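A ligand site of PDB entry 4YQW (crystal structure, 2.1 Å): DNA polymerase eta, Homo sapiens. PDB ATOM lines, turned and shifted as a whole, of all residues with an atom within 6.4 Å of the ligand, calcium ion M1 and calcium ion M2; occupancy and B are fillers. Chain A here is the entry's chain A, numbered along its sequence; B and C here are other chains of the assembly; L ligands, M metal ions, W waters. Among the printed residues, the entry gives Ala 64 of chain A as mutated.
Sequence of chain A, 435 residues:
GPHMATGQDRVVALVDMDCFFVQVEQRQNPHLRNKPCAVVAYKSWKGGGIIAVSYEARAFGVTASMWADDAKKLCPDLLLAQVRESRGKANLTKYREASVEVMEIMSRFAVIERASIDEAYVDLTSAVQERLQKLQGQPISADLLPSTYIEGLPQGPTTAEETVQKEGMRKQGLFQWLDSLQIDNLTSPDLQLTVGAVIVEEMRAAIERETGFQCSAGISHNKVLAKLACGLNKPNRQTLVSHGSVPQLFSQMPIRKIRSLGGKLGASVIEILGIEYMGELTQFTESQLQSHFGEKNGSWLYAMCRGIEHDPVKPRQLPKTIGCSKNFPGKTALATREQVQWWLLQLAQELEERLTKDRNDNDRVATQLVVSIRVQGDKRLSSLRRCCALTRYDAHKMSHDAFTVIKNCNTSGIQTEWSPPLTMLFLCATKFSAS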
ATOM      1  N   ASP A  16     -15.049   0.796 -35.347  1.00  0.00           N
ATOM      2  CA  ASP A  16     -14.511   0.913 -33.985  1.00  0.00           C
ATOM      3  C   ASP A  16     -15.150   2.071 -33.203  1.00  0.00           C
ATOM      4  O   ASP A  16     -15.187   3.195 -33.675  1.00  0.00           O
ATOM      5  CB  ASP A  16     -12.994   1.098 -34.049  1.00  0.00           C
ATOM      6  CG  ASP A  16     -12.431   1.609 -32.745  1.00  0.00           C
ATOM      7  OD1 ASP A  16     -12.357   2.839 -32.555  1.00  0.00           O
ATOM      8  OD2 ASP A  16     -12.041   0.791 -31.899  1.00  0.00           O
ATOM      9  N   MET A  17     -15.624   1.811 -31.993  1.00  0.00           N
ATOM     10  CA  MET A  17     -16.304   2.839 -31.220  1.00  0.00           C
ATOM     11  C   MET A  17     -15.313   3.912 -30.738  1.00  0.00           C
ATOM     12  O   MET A  17     -14.183   3.614 -30.381  1.00  0.00           O
ATOM     13  CB  MET A  17     -17.030   2.212 -30.021  1.00  0.00           C
ATOM     14  CG  MET A  17     -17.816   0.942 -30.383  1.00  0.00           C
ATOM     15  SD  MET A  17     -19.074   1.284 -31.645  1.00  0.00           S
ATOM     16  CE  MET A  17     -20.094   2.463 -30.787  1.00  0.00           C
ATOM     17  N   ASP A  18     -15.757   5.158 -30.753  1.00  0.00           N
ATOM     18  CA  ASP A  18     -14.934   6.264 -30.264  1.00  0.00           C
ATOM     19  C   ASP A  18     -14.878   6.244 -28.735  1.00  0.00           C
ATOM     20  O   ASP A  18     -15.919   6.062 -28.105  1.00  0.00           O
ATOM     21  CB  ASP A  18     -15.500   7.610 -30.760  1.00  0.00           C
ATOM     22  CG  ASP A  18     -15.498   7.724 -32.277  1.00  0.00           C
ATOM     23  OD1 ASP A  18     -14.621   7.113 -32.914  1.00  0.00           O
ATOM     24  OD2 ASP A  18     -16.372   8.419 -32.840  1.00  0.00           O
ATOM     25  N   CYS A  19     -13.683   6.441 -28.167  1.00  0.00           N
ATOM     26  CA  CYS A  19     -13.412   6.409 -26.725  1.00  0.00           C
ATOM     27  C   CYS A  19     -14.465   5.615 -25.934  1.00  0.00           C
ATOM     28  O   CYS A  19     -15.220   6.182 -25.145  1.00  0.00           O
ATOM     29  CB  CYS A  19     -13.304   7.837 -26.156  1.00  0.00           C
ATOM     30  SG  CYS A  19     -14.643   9.015 -26.533  1.00  0.00           S
ATOM     31  N   PHE A  20     -14.497   4.313 -26.169  1.00  0.00           N
ATOM     32  CA  PHE A  20     -15.690   3.521 -25.861  1.00  0.00           C
ATOM     33  C   PHE A  20     -16.132   3.547 -24.396  1.00  0.00           C
ATOM     34  O   PHE A  20     -17.300   3.831 -24.125  1.00  0.00           O
ATOM     35  CB  PHE A  20     -15.470   2.085 -26.321  1.00  0.00           C
ATOM     36  CG  PHE A  20     -16.678   1.205 -26.143  1.00  0.00           C
ATOM     37  CD1 PHE A  20     -17.917   1.590 -26.658  1.00  0.00           C
ATOM     38  CD2 PHE A  20     -16.588   0.008 -25.441  1.00  0.00           C
ATOM     39  CE1 PHE A  20     -19.037   0.797 -26.481  1.00  0.00           C
ATOM     40  CE2 PHE A  20     -17.719  -0.812 -25.277  1.00  0.00           C
ATOM     41  CZ  PHE A  20     -18.940  -0.400 -25.801  1.00  0.00           C
ATOM     42  N   PHE A  21     -15.240   3.234 -23.449  1.00  0.00           N
ATOM     43  CA  PHE A  21     -15.703   3.138 -22.047  1.00  0.00           C
ATOM     44  C   PHE A  21     -16.223   4.508 -21.611  1.00  0.00           C
ATOM     45  O   PHE A  21     -17.167   4.600 -20.831  1.00  0.00           O
ATOM     46  CB  PHE A  21     -14.611   2.655 -21.091  1.00  0.00           C
ATOM     47  CG  PHE A  21     -14.282   1.181 -21.206  1.00  0.00           C
ATOM     48  CD1 PHE A  21     -14.670   0.428 -22.312  1.00  0.00           C
ATOM     49  CD2 PHE A  21     -13.535   0.564 -20.216  1.00  0.00           C
ATOM     50  CE1 PHE A  21     -14.341  -0.911 -22.413  1.00  0.00           C
ATOM     51  CE2 PHE A  21     -13.201  -0.781 -20.310  1.00  0.00           C
ATOM     52  CZ  PHE A  21     -13.596  -1.519 -21.400  1.00  0.00           C
ATOM     53  N   VAL A  22     -15.636   5.573 -22.156  1.00  0.00           N
ATOM     54  CA  VAL A  22     -16.061   6.935 -21.829  1.00  0.00           C
ATOM     55  C   VAL A  22     -17.487   7.229 -22.344  1.00  0.00           C
ATOM     56  O   VAL A  22     -18.321   7.723 -21.593  1.00  0.00           O
ATOM     57  CB  VAL A  22     -15.074   7.965 -22.387  1.00  0.00           C
ATOM     58  CG1 VAL A  22     -15.713   9.315 -22.408  1.00  0.00           C
ATOM     59  CG2 VAL A  22     -13.773   8.002 -21.536  1.00  0.00           C
ATOM     60  N   ILE A  51      -8.034   4.456 -18.184  1.00  0.00           N
ATOM     61  CA  ILE A  51      -8.189   3.348 -19.107  1.00  0.00           C
ATOM     62  C   ILE A  51      -8.794   3.829 -20.416  1.00  0.00           C
ATOM     63  O   ILE A  51      -8.725   3.130 -21.439  1.00  0.00           O
ATOM     64  CB  ILE A  51      -9.061   2.242 -18.460  1.00  0.00           C
ATOM     65  CG1 ILE A  51      -9.108   0.978 -19.307  1.00  0.00           C
ATOM     66  CG2 ILE A  51     -10.491   2.720 -18.221  1.00  0.00           C
ATOM     67  CD1 ILE A  51     -10.188   0.040 -18.813  1.00  0.00           C
ATOM     68  N   ALA A  52      -9.392   5.026 -20.379  1.00  0.00           N
ATOM     69  CA  ALA A  52     -10.082   5.586 -21.531  1.00  0.00           C
ATOM     70  C   ALA A  52     -10.264   7.092 -21.358  1.00  0.00           C
ATOM     71  O   ALA A  52     -10.533   7.567 -20.248  1.00  0.00           O
ATOM     72  CB  ALA A  52     -11.447   4.898 -21.736  1.00  0.00           C
ATOM     73  N   VAL A  53     -10.162   7.836 -22.469  1.00  0.00           N
ATOM     74  CA  VAL A  53     -10.052   9.296 -22.426  1.00  0.00           C
ATOM     75  C   VAL A  53     -10.901   9.946 -23.518  1.00  0.00           C
ATOM     76  O   VAL A  53     -10.736   9.636 -24.703  1.00  0.00           O
ATOM     77  CB  VAL A  53      -8.574   9.739 -22.632  1.00  0.00           C
ATOM     78  CG1 VAL A  53      -8.447  11.250 -22.415  1.00  0.00           C
ATOM     79  CG2 VAL A  53      -7.662   9.004 -21.714  1.00  0.00           C
ATOM     80  N   TYR A  55     -12.207  12.795 -26.228  1.00  0.00           N
ATOM     81  CA  TYR A  55     -11.411  13.601 -27.150  1.00  0.00           C
ATOM     82  C   TYR A  55     -11.180  15.032 -26.601  1.00  0.00           C
ATOM     83  O   TYR A  55     -10.127  15.612 -26.845  1.00  0.00           O
ATOM     84  CB  TYR A  55     -12.061  13.620 -28.542  1.00  0.00           C
ATOM     85  CG  TYR A  55     -11.758  12.329 -29.268  1.00  0.00           C
ATOM     86  CD1 TYR A  55     -12.478  11.166 -28.992  1.00  0.00           C
ATOM     87  CD2 TYR A  55     -10.723  12.250 -30.183  1.00  0.00           C
ATOM     88  CE1 TYR A  55     -12.179   9.960 -29.633  1.00  0.00           C
ATOM     89  CE2 TYR A  55     -10.413  11.061 -30.821  1.00  0.00           C
ATOM     90  CZ  TYR A  55     -11.150   9.911 -30.551  1.00  0.00           C
ATOM     91  OH  TYR A  55     -10.822   8.734 -31.193  1.00  0.00           O
ATOM     92  N   ARG A  58      -8.210  14.569 -24.426  1.00  0.00           N
ATOM     93  CA  ARG A  58      -7.001  14.313 -25.212  1.00  0.00           C
ATOM     94  C   ARG A  58      -6.385  15.636 -25.715  1.00  0.00           C
ATOM     95  O   ARG A  58      -5.176  15.725 -25.938  1.00  0.00           O
ATOM     96  CB  ARG A  58      -7.281  13.374 -26.398  1.00  0.00           C
ATOM     97  CG  ARG A  58      -7.769  11.980 -25.991  1.00  0.00           C
ATOM     98  CD  ARG A  58      -8.035  11.088 -27.211  1.00  0.00           C
ATOM     99  NE  ARG A  58      -8.894   9.956 -26.847  1.00  0.00           N
ATOM    100  CZ  ARG A  58      -9.096   8.884 -27.603  1.00  0.00           C
ATOM    101  NH1 ARG A  58      -8.510   8.787 -28.803  1.00  0.00           N
ATOM    102  NH2 ARG A  58      -9.888   7.914 -27.165  1.00  0.00           N
ATOM    103  N   ALA A  64      -4.353   7.370 -21.922  1.00  0.00           N
ATOM    104  CA  ALA A  64      -4.460   6.138 -21.154  1.00  0.00           C
ATOM    105  C   ALA A  64      -3.097   5.776 -20.583  1.00  0.00           C
ATOM    106  O   ALA A  64      -2.069   6.261 -21.059  1.00  0.00           O
ATOM    107  CB  ALA A  64      -5.001   4.997 -22.024  1.00  0.00           C
ATOM    108  N   LEU A  92     -15.950  -5.467 -15.649  1.00  0.00           N
ATOM    109  CA  LEU A  92     -16.184  -4.807 -16.933  1.00  0.00           C
ATOM    110  C   LEU A  92     -17.570  -5.075 -17.525  1.00  0.00           C
ATOM    111  O   LEU A  92     -17.828  -4.726 -18.672  1.00  0.00           O
ATOM    112  CB  LEU A  92     -15.118  -5.227 -17.942  1.00  0.00           C
ATOM    113  CG  LEU A  92     -13.695  -5.125 -17.402  1.00  0.00           C
ATOM    114  CD1 LEU A  92     -12.697  -5.614 -18.441  1.00  0.00           C
ATOM    115  CD2 LEU A  92     -13.397  -3.689 -16.991  1.00  0.00           C
ATOM    116  N   SER A 116     -12.742  -7.109 -30.882  1.00  0.00           N
ATOM    117  CA  SER A 116     -12.455  -6.672 -29.524  1.00  0.00           C
ATOM    118  C   SER A 116     -13.757  -6.233 -28.880  1.00  0.00           C
ATOM    119  O   SER A 116     -14.808  -6.295 -29.517  1.00  0.00           O
ATOM    120  CB  SER A 116     -11.438  -5.521 -29.508  1.00  0.00           C
ATOM    121  OG  SER A 116     -12.086  -4.264 -29.651  1.00  0.00           O
ATOM    122  N   ILE A 117     -13.713  -5.802 -27.618  1.00  0.00           N
ATOM    123  CA  ILE A 117     -14.928  -5.326 -26.970  1.00  0.00           C
ATOM    124  C   ILE A 117     -15.624  -4.184 -27.773  1.00  0.00           C
ATOM    125  O   ILE A 117     -16.866  -4.054 -27.711  1.00  0.00           O
ATOM    126  CB  ILE A 117     -14.647  -4.854 -25.520  1.00  0.00           C
ATOM    127  CG1 ILE A 117     -15.926  -4.847 -24.677  1.00  0.00           C
ATOM    128  CG2 ILE A 117     -13.940  -3.493 -25.501  1.00  0.00           C
ATOM    129  CD1 ILE A 117     -15.663  -4.682 -23.197  1.00  0.00           C
ATOM    130  N   ASP A 118     -14.875  -3.391 -28.536  1.00  0.00           N
ATOM    131  CA  ASP A 118     -15.504  -2.259 -29.221  1.00  0.00           C
ATOM    132  C   ASP A 118     -15.225  -2.183 -30.732  1.00  0.00           C
ATOM    133  O   ASP A 118     -15.462  -1.137 -31.345  1.00  0.00           O
ATOM    134  CB  ASP A 118     -15.103  -0.938 -28.548  1.00  0.00           C
ATOM    135  CG  ASP A 118     -13.747  -0.420 -29.002  1.00  0.00           C
ATOM    136  OD1 ASP A 118     -12.847  -1.224 -29.330  1.00  0.00           O
ATOM    137  OD2 ASP A 118     -13.592   0.814 -29.049  1.00  0.00           O
ATOM    138  N   GLU A 119     -14.749  -3.275 -31.335  1.00  0.00           N
ATOM    139  CA  GLU A 119     -14.482  -3.330 -32.774  1.00  0.00           C
ATOM    140  C   GLU A 119     -14.999  -4.582 -33.438  1.00  0.00           C
ATOM    141  O   GLU A 119     -14.905  -5.668 -32.862  1.00  0.00           O
ATOM    142  CB  GLU A 119     -12.984  -3.255 -33.087  1.00  0.00           C
ATOM    143  CG  GLU A 119     -12.186  -2.288 -32.269  1.00  0.00           C
ATOM    144  CD  GLU A 119     -10.739  -2.267 -32.687  1.00  0.00           C
ATOM    145  OE1 GLU A 119     -10.293  -3.282 -33.252  1.00  0.00           O
ATOM    146  OE2 GLU A 119     -10.059  -1.247 -32.494  1.00  0.00           O
ATOM    147  N   LYS A 227      -8.796  -1.615 -41.172  1.00  0.00           N
ATOM    148  CA  LYS A 227      -8.316  -1.198 -39.846  1.00  0.00           C
ATOM    149  C   LYS A 227      -7.453   0.083 -39.921  1.00  0.00           C
ATOM    150  O   LYS A 227      -7.676   1.021 -39.159  1.00  0.00           O
ATOM    151  CB  LYS A 227      -7.552  -2.346 -39.189  1.00  0.00           C
ATOM    152  CG  LYS A 227      -6.784  -1.984 -37.937  1.00  0.00           C
ATOM    153  CD  LYS A 227      -7.656  -2.035 -36.716  1.00  0.00           C
ATOM    154  CE  LYS A 227      -6.844  -1.783 -35.449  1.00  0.00           C
ATOM    155  NZ  LYS A 227      -7.717  -1.090 -34.441  1.00  0.00           N
ATOM    156  N   LYS A 234     -10.630  10.136 -37.108  1.00  0.00           N
ATOM    157  CA  LYS A 234     -11.388   9.866 -35.891  1.00  0.00           C
ATOM    158  C   LYS A 234     -11.513  11.177 -35.157  1.00  0.00           C
ATOM    159  O   LYS A 234     -10.654  12.041 -35.312  1.00  0.00           O
ATOM    160  CB  LYS A 234     -10.685   8.815 -35.009  1.00  0.00           C
ATOM    161  CG  LYS A 234     -11.077   7.376 -35.319  1.00  0.00           C
ATOM    162  CD  LYS A 234     -10.399   6.348 -34.399  1.00  0.00           C
ATOM    163  CE  LYS A 234     -11.090   6.179 -33.054  1.00  0.00           C
ATOM    164  NZ  LYS A 234     -12.339   5.323 -33.032  1.00  0.00           N
ATOM    165  N   PRO A 235     -12.599  11.375 -34.392  1.00  0.00           N
ATOM    166  CA  PRO A 235     -13.759  10.499 -34.159  1.00  0.00           C
ATOM    167  C   PRO A 235     -14.948  10.771 -35.083  1.00  0.00           C
ATOM    168  O   PRO A 235     -14.913  11.709 -35.874  1.00  0.00           O
ATOM    169  CB  PRO A 235     -14.122  10.821 -32.707  1.00  0.00           C
ATOM    170  CG  PRO A 235     -13.801  12.318 -32.607  1.00  0.00           C
ATOM    171  CD  PRO A 235     -12.635  12.571 -33.533  1.00  0.00           C
ATOM    172  P    DT B   8      -4.945  -2.012 -31.232  1.00  0.00           P
ATOM    173  OP1  DT B   8      -5.561  -1.240 -32.339  1.00  0.00           O
ATOM    174  OP2  DT B   8      -3.903  -1.375 -30.384  1.00  0.00           O
ATOM    175  O5'  DT B   8      -6.151  -2.531 -30.273  1.00  0.00           O
ATOM    176  C5'  DT B   8      -7.268  -3.303 -30.810  1.00  0.00           C
ATOM    177  C4'  DT B   8      -8.349  -3.480 -29.759  1.00  0.00           C
ATOM    178  O4'  DT B   8      -7.828  -4.191 -28.621  1.00  0.00           O
ATOM    179  C3'  DT B   8      -8.942  -2.183 -29.203  1.00  0.00           C
ATOM    180  O3'  DT B   8     -10.323  -2.384 -28.931  1.00  0.00           O
ATOM    181  C2'  DT B   8      -8.137  -1.967 -27.914  1.00  0.00           C
ATOM    182  C1'  DT B   8      -7.971  -3.421 -27.442  1.00  0.00           C
ATOM    183  N1   DT B   8      -6.761  -3.663 -26.554  1.00  0.00           N
ATOM    184  C2   DT B   8      -6.941  -4.219 -25.298  1.00  0.00           C
ATOM    185  O2   DT B   8      -8.040  -4.508 -24.854  1.00  0.00           O
ATOM    186  N3   DT B   8      -5.795  -4.417 -24.581  1.00  0.00           N
ATOM    187  C4   DT B   8      -4.508  -4.124 -24.974  1.00  0.00           C
ATOM    188  O4   DT B   8      -3.554  -4.324 -24.242  1.00  0.00           O
ATOM    189  C5   DT B   8      -4.371  -3.537 -26.293  1.00  0.00           C
ATOM    190  C7   DT B   8      -3.017  -3.165 -26.814  1.00  0.00           C
ATOM    191  C6   DT B   8      -5.488  -3.334 -27.015  1.00  0.00           C
ATOM    192  P    DT C   3       1.203   1.089 -16.256  1.00  0.00           P
ATOM    193  OP1  DT C   3       0.694  -0.269 -15.952  1.00  0.00           O
ATOM    194  OP2  DT C   3       1.421   1.487 -17.663  1.00  0.00           O
ATOM    195  O5'  DT C   3       0.274   2.184 -15.547  1.00  0.00           O
ATOM    196  C5'  DT C   3      -0.878   2.700 -16.208  1.00  0.00           C
ATOM    197  C4'  DT C   3      -2.141   2.227 -15.511  1.00  0.00           C
ATOM    198  O4'  DT C   3      -3.288   2.398 -16.398  1.00  0.00           O
ATOM    199  C3'  DT C   3      -2.119   0.769 -15.121  1.00  0.00           C
ATOM    200  O3'  DT C   3      -2.433   0.578 -13.716  1.00  0.00           O
ATOM    201  C2'  DT C   3      -3.061   0.036 -16.091  1.00  0.00           C
ATOM    202  C1'  DT C   3      -3.740   1.154 -16.897  1.00  0.00           C
ATOM    203  N1   DT C   3      -3.460   1.107 -18.370  1.00  0.00           N
ATOM    204  C2   DT C   3      -4.502   1.302 -19.245  1.00  0.00           C
ATOM    205  O2   DT C   3      -5.643   1.508 -18.878  1.00  0.00           O
ATOM    206  N3   DT C   3      -4.151   1.260 -20.562  1.00  0.00           N
ATOM    207  C4   DT C   3      -2.891   1.036 -21.081  1.00  0.00           C
ATOM    208  O4   DT C   3      -2.680   1.011 -22.290  1.00  0.00           O
ATOM    209  C5   DT C   3      -1.843   0.832 -20.114  1.00  0.00           C
ATOM    210  C7   DT C   3      -0.431   0.572 -20.557  1.00  0.00           C
ATOM    211  C6   DT C   3      -2.175   0.875 -18.810  1.00  0.00           C
ATOM    212  P    DG C   4      -0.908  -2.185 -13.324  1.00  0.00           P
ATOM    213  OP1  DG C   4      -1.021  -2.703 -11.942  1.00  0.00           O
ATOM    214  OP2  DG C   4      -0.391  -3.058 -14.399  1.00  0.00           O
ATOM    215  O5'  DG C   4      -2.405  -1.827 -13.718  1.00  0.00           O
ATOM    216  C5'  DG C   4      -3.365  -1.563 -12.690  1.00  0.00           C
ATOM    217  C4'  DG C   4      -4.710  -2.164 -13.080  1.00  0.00           C
ATOM    218  O4'  DG C   4      -4.928  -1.950 -14.497  1.00  0.00           O
ATOM    219  C3'  DG C   4      -4.807  -3.678 -12.908  1.00  0.00           C
ATOM    220  O3'  DG C   4      -6.182  -4.051 -12.906  1.00  0.00           O
ATOM    221  C2'  DG C   4      -4.144  -4.151 -14.191  1.00  0.00           C
ATOM    222  C1'  DG C   4      -4.820  -3.202 -15.159  1.00  0.00           C
ATOM    223  N9   DG C   4      -4.117  -3.008 -16.421  1.00  0.00           N
ATOM    224  C8   DG C   4      -2.762  -3.101 -16.691  1.00  0.00           C
ATOM    225  N7   DG C   4      -2.481  -2.854 -17.952  1.00  0.00           N
ATOM    226  C5   DG C   4      -3.712  -2.588 -18.522  1.00  0.00           C
ATOM    227  C6   DG C   4      -4.074  -2.252 -19.851  1.00  0.00           C
ATOM    228  O6   DG C   4      -3.327  -2.122 -20.839  1.00  0.00           O
ATOM    229  N1   DG C   4      -5.453  -2.060 -19.976  1.00  0.00           N
ATOM    230  C2   DG C   4      -6.354  -2.178 -18.932  1.00  0.00           C
ATOM    231  N2   DG C   4      -7.635  -1.976 -19.199  1.00  0.00           N
ATOM    232  N3   DG C   4      -6.025  -2.493 -17.709  1.00  0.00           N
ATOM    233  C4   DG C   4      -4.716  -2.674 -17.580  1.00  0.00           C
ATOM    234  P    DA C   5      -6.605  -5.599 -12.712  1.00  0.00           P
ATOM    235  OP1  DA C   5      -7.645  -5.584 -11.650  1.00  0.00           O
ATOM    236  OP2  DA C   5      -5.389  -6.434 -12.599  1.00  0.00           O
ATOM    237  O5'  DA C   5      -7.430  -5.939 -14.051  1.00  0.00           O
ATOM    238  C5'  DA C   5      -8.719  -5.360 -14.245  1.00  0.00           C
ATOM    239  C4'  DA C   5      -9.314  -5.767 -15.578  1.00  0.00           C
ATOM    240  O4'  DA C   5      -8.459  -5.272 -16.652  1.00  0.00           O
ATOM    241  C3'  DA C   5      -9.425  -7.292 -15.789  1.00  0.00           C
ATOM    242  O3'  DA C   5     -10.689  -7.612 -16.309  1.00  0.00           O
ATOM    243  C2'  DA C   5      -8.312  -7.600 -16.777  1.00  0.00           C
ATOM    244  C1'  DA C   5      -8.266  -6.304 -17.582  1.00  0.00           C
ATOM    245  N9   DA C   5      -7.001  -6.108 -18.273  1.00  0.00           N
ATOM    246  C8   DA C   5      -5.746  -6.335 -17.796  1.00  0.00           C
ATOM    247  N7   DA C   5      -4.796  -6.097 -18.682  1.00  0.00           N
ATOM    248  C5   DA C   5      -5.489  -5.712 -19.818  1.00  0.00           C
ATOM    249  C6   DA C   5      -5.073  -5.334 -21.100  1.00  0.00           C
ATOM    250  N6   DA C   5      -3.790  -5.278 -21.481  1.00  0.00           N
ATOM    251  N1   DA C   5      -6.026  -5.013 -21.993  1.00  0.00           N
ATOM    252  C2   DA C   5      -7.303  -5.048 -21.615  1.00  0.00           C
ATOM    253  N3   DA C   5      -7.827  -5.400 -20.452  1.00  0.00           N
ATOM    254  C4   DA C   5      -6.849  -5.722 -19.579  1.00  0.00           C
HETATM  255  N1  LIG L   1      -8.955  -0.604 -23.346  1.00  0.00           N
HETATM  256  C1  LIG L   1      -8.343  -1.211 -22.243  1.00  0.00           C
HETATM  257  N2  LIG L   1      -7.010  -1.425 -22.218  1.00  0.00           N
HETATM  258  C2  LIG L   1      -6.255  -1.059 -23.284  1.00  0.00           C
HETATM  259  C3  LIG L   1      -6.855  -0.448 -24.393  1.00  0.00           C
HETATM  260  C4  LIG L   1      -8.224  -0.225 -24.397  1.00  0.00           C
HETATM  261  O1  LIG L   1      -9.105  -1.530 -21.314  1.00  0.00           O
HETATM  262  N3  LIG L   1      -4.908  -1.239 -23.288  1.00  0.00           N
HETATM  263  C5  LIG L   1     -10.423  -0.428 -23.265  1.00  0.00           C
HETATM  264  C6  LIG L   1     -10.780   1.033 -22.990  1.00  0.00           C
HETATM  265  C7  LIG L   1     -11.277   1.546 -24.344  1.00  0.00           C
HETATM  266  C8  LIG L   1     -11.773   0.303 -25.061  1.00  0.00           C
HETATM  267  O2  LIG L   1     -10.993  -0.780 -24.530  1.00  0.00           O
HETATM  268  O3  LIG L   1     -12.300   2.531 -24.226  1.00  0.00           O
HETATM  269  C9  LIG L   1     -11.512   0.414 -26.561  1.00  0.00           C
HETATM  270  O4  LIG L   1     -10.102   0.612 -26.738  1.00  0.00           O
HETATM  271  P1  LIG L   1      -9.546   1.502 -27.959  1.00  0.00           P
HETATM  272  O5  LIG L   1     -10.491   1.399 -29.125  1.00  0.00           O
HETATM  273  O6  LIG L   1      -8.095   1.185 -28.149  1.00  0.00           O
HETATM  274  O7  LIG L   1      -9.659   3.006 -27.351  1.00  0.00           O
HETATM  275  P2  LIG L   1     -11.002   3.910 -27.297  1.00  0.00           P
HETATM  276  O8  LIG L   1     -12.167   3.236 -27.959  1.00  0.00           O
HETATM  277  O9  LIG L   1     -11.149   4.367 -25.866  1.00  0.00           O
HETATM  278  O10 LIG L   1     -10.534   5.237 -28.097  1.00  0.00           O
HETATM  279  P3  LIG L   1     -10.462   5.430 -29.697  1.00  0.00           P
HETATM  280  O11 LIG L   1     -10.678   4.073 -30.291  1.00  0.00           O
HETATM  281  O12 LIG L   1     -11.540   6.468 -29.941  1.00  0.00           O
HETATM  282  O13 LIG L   1      -9.028   5.907 -29.858  1.00  0.00           O
HETATM  283 CA    CA M   1     -12.195   2.438 -30.095  1.00  0.00          CA
HETATM  284 CA    CA M   2     -10.885  -0.655 -30.501  1.00  0.00          CA
HETATM  285  O   HOH W   1      -6.630   1.555 -22.004  1.00  0.00           O
HETATM  286  O   HOH W   2     -10.625  -3.573 -20.227  1.00  0.00           O
HETATM  287  O   HOH W   3      -9.563   6.202 -24.670  1.00  0.00           O
HETATM  288  O   HOH W   4      -8.642   3.173 -31.744  1.00  0.00           O
HETATM  289  O   HOH W   5      -3.656   0.221 -25.697  1.00  0.00           O
HETATM  290  O   HOH W   6      -6.903   5.708 -28.555  1.00  0.00           O
HETATM  291  O   HOH W   7      -8.908   0.585 -31.286  1.00  0.00           O
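N of Phe 21 is in hydrogen-bond range of O3 of the ligand (3.1 Å). O6 of DG 4 of chain C lies within hydrogen-bond range of N3 of the ligand (3.0 Å). N of Phe 20 lies within hydrogen-bond range of O9 of the ligand, at 3.4 Å. O4 of DT 3 of chain C sits at hydrogen-bond distance from N3 of the ligand (3.3 Å). NH1 of Arg 58 is in salt-bridge range of O13 of the ligand, 3.1 Å away. The side-chain amino group of Lys 234 lies within salt-bridge range of an oxygen (O12) of the ligand (3.4 Å). An oxygen (O12) of the ligand sits at hydrogen-bond distance from the side-chain hydroxyl (OH) of Tyr 55, at 2.7 Å. The backbone NH of Cys 19 is in hydrogen-bond range of an oxygen (O12) of the ligand.
Water W6 bridges an oxygen (O13) of the ligand (2.5 Å) and the guanidinium group of Arg 58 (3.5 Å). Water W3 lies within hydrogen-bond range of O9 of the ligand, N of Val 53 and NH2 of Arg 58. Water W2 lies within hydrogen-bond range of O1 of the ligand and N3 of DA 5 of chain C.
Three residues have an atom within 4 Å of calcium ion M1: Asp 16, Met 17 and Asp 118. Along chain A the residues within 4 Å of calcium ion M1 span positions 16 to 118.
Asp 18 touches the ligand. Ile 51 touches the ligand (CD1 to O1, 3.1 Å). CB of Ala 52 touches O3 of the ligand (3.5 Å). C2 of DA 5 of chain C touches N2 of the ligand (3.7 Å). 16 residues have an atom within 4 Å of the ligand: Asp 16, Met 17, Asp 18, Cys 19, Phe 20, Phe 21, Ile 51, Ala 52, Tyr 55, Arg 58, Asp 118, Lys 234, DT 8 of chain B, DT 3 of chain C, DG 4 of chain C and DA 5 of chain C.
Residues that only touch calcium ion M2: Ser 116 (3.9 Å). Within 4 Å of calcium ion M2: Asp 16, Ser 116, Asp 118, Glu 119 and DT 8 of chain B. Along chain A the residues within 4 Å of calcium ion M2 span positions 16 to 119.
Calcium ion M1 is bound by an oxygen (O5) of the ligand (2.2 Å), an oxygen (O11) of the ligand (2.2 Å), an oxygen (O8) of the ligand (2.3 Å), the backbone carbonyl oxygen (O) of Met 17 (2.3 Å), the side-chain carboxylate (OD2) of Asp 118 (2.4 Å), the side-chain carboxylate (OD2) of Asp 16 (2.4 Å) and the side-chain carboxylate (OD1) of Asp 16 (2.5 Å). Calcium ion M1 has seven donor atoms within binding distance.
The side-chain carboxylate of Asp 16 lies close to the side-chain amino group of Lys 234 (2.5 Å). OG of Ser 116 sits close to N of Asp 118, 3.1 Å away. The side-chain hydroxyl of Ser 116 lies close to the backbone NH of Glu 119, 3.3 Å away. The side-chain carboxylate (OD1) of Asp 18 lies within salt-bridge range of the side-chain amino group (NZ) of Lys 234 (2.9 Å). O3' of DT 8 of chain B lies close to the side-chain hydroxyl (OG) of Ser 116 (2.7 Å). The side-chain hydroxyl of Tyr 55 is in hydrogen-bond range of the guanidinium group of Arg 58, at 3.3 Å. The side-chain amino group of Lys 227 lies within salt-bridge range of the side-chain carboxylate of Glu 119, 3.6 Å away. OP1 of DT 8 of chain B is in salt-bridge range of the side-chain amino group of Lys 227, 3.0 Å away.
Calcium ion M2 is bound by OE2 of Glu 119 (2.2 Å), OD2 of Asp 16 (2.3 Å), OD1 of Asp 118 (2.4 Å), O3' of DT 8 of chain B (2.4 Å), water W7 (2.5 Å) and O5 of the ligand (2.5 Å).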
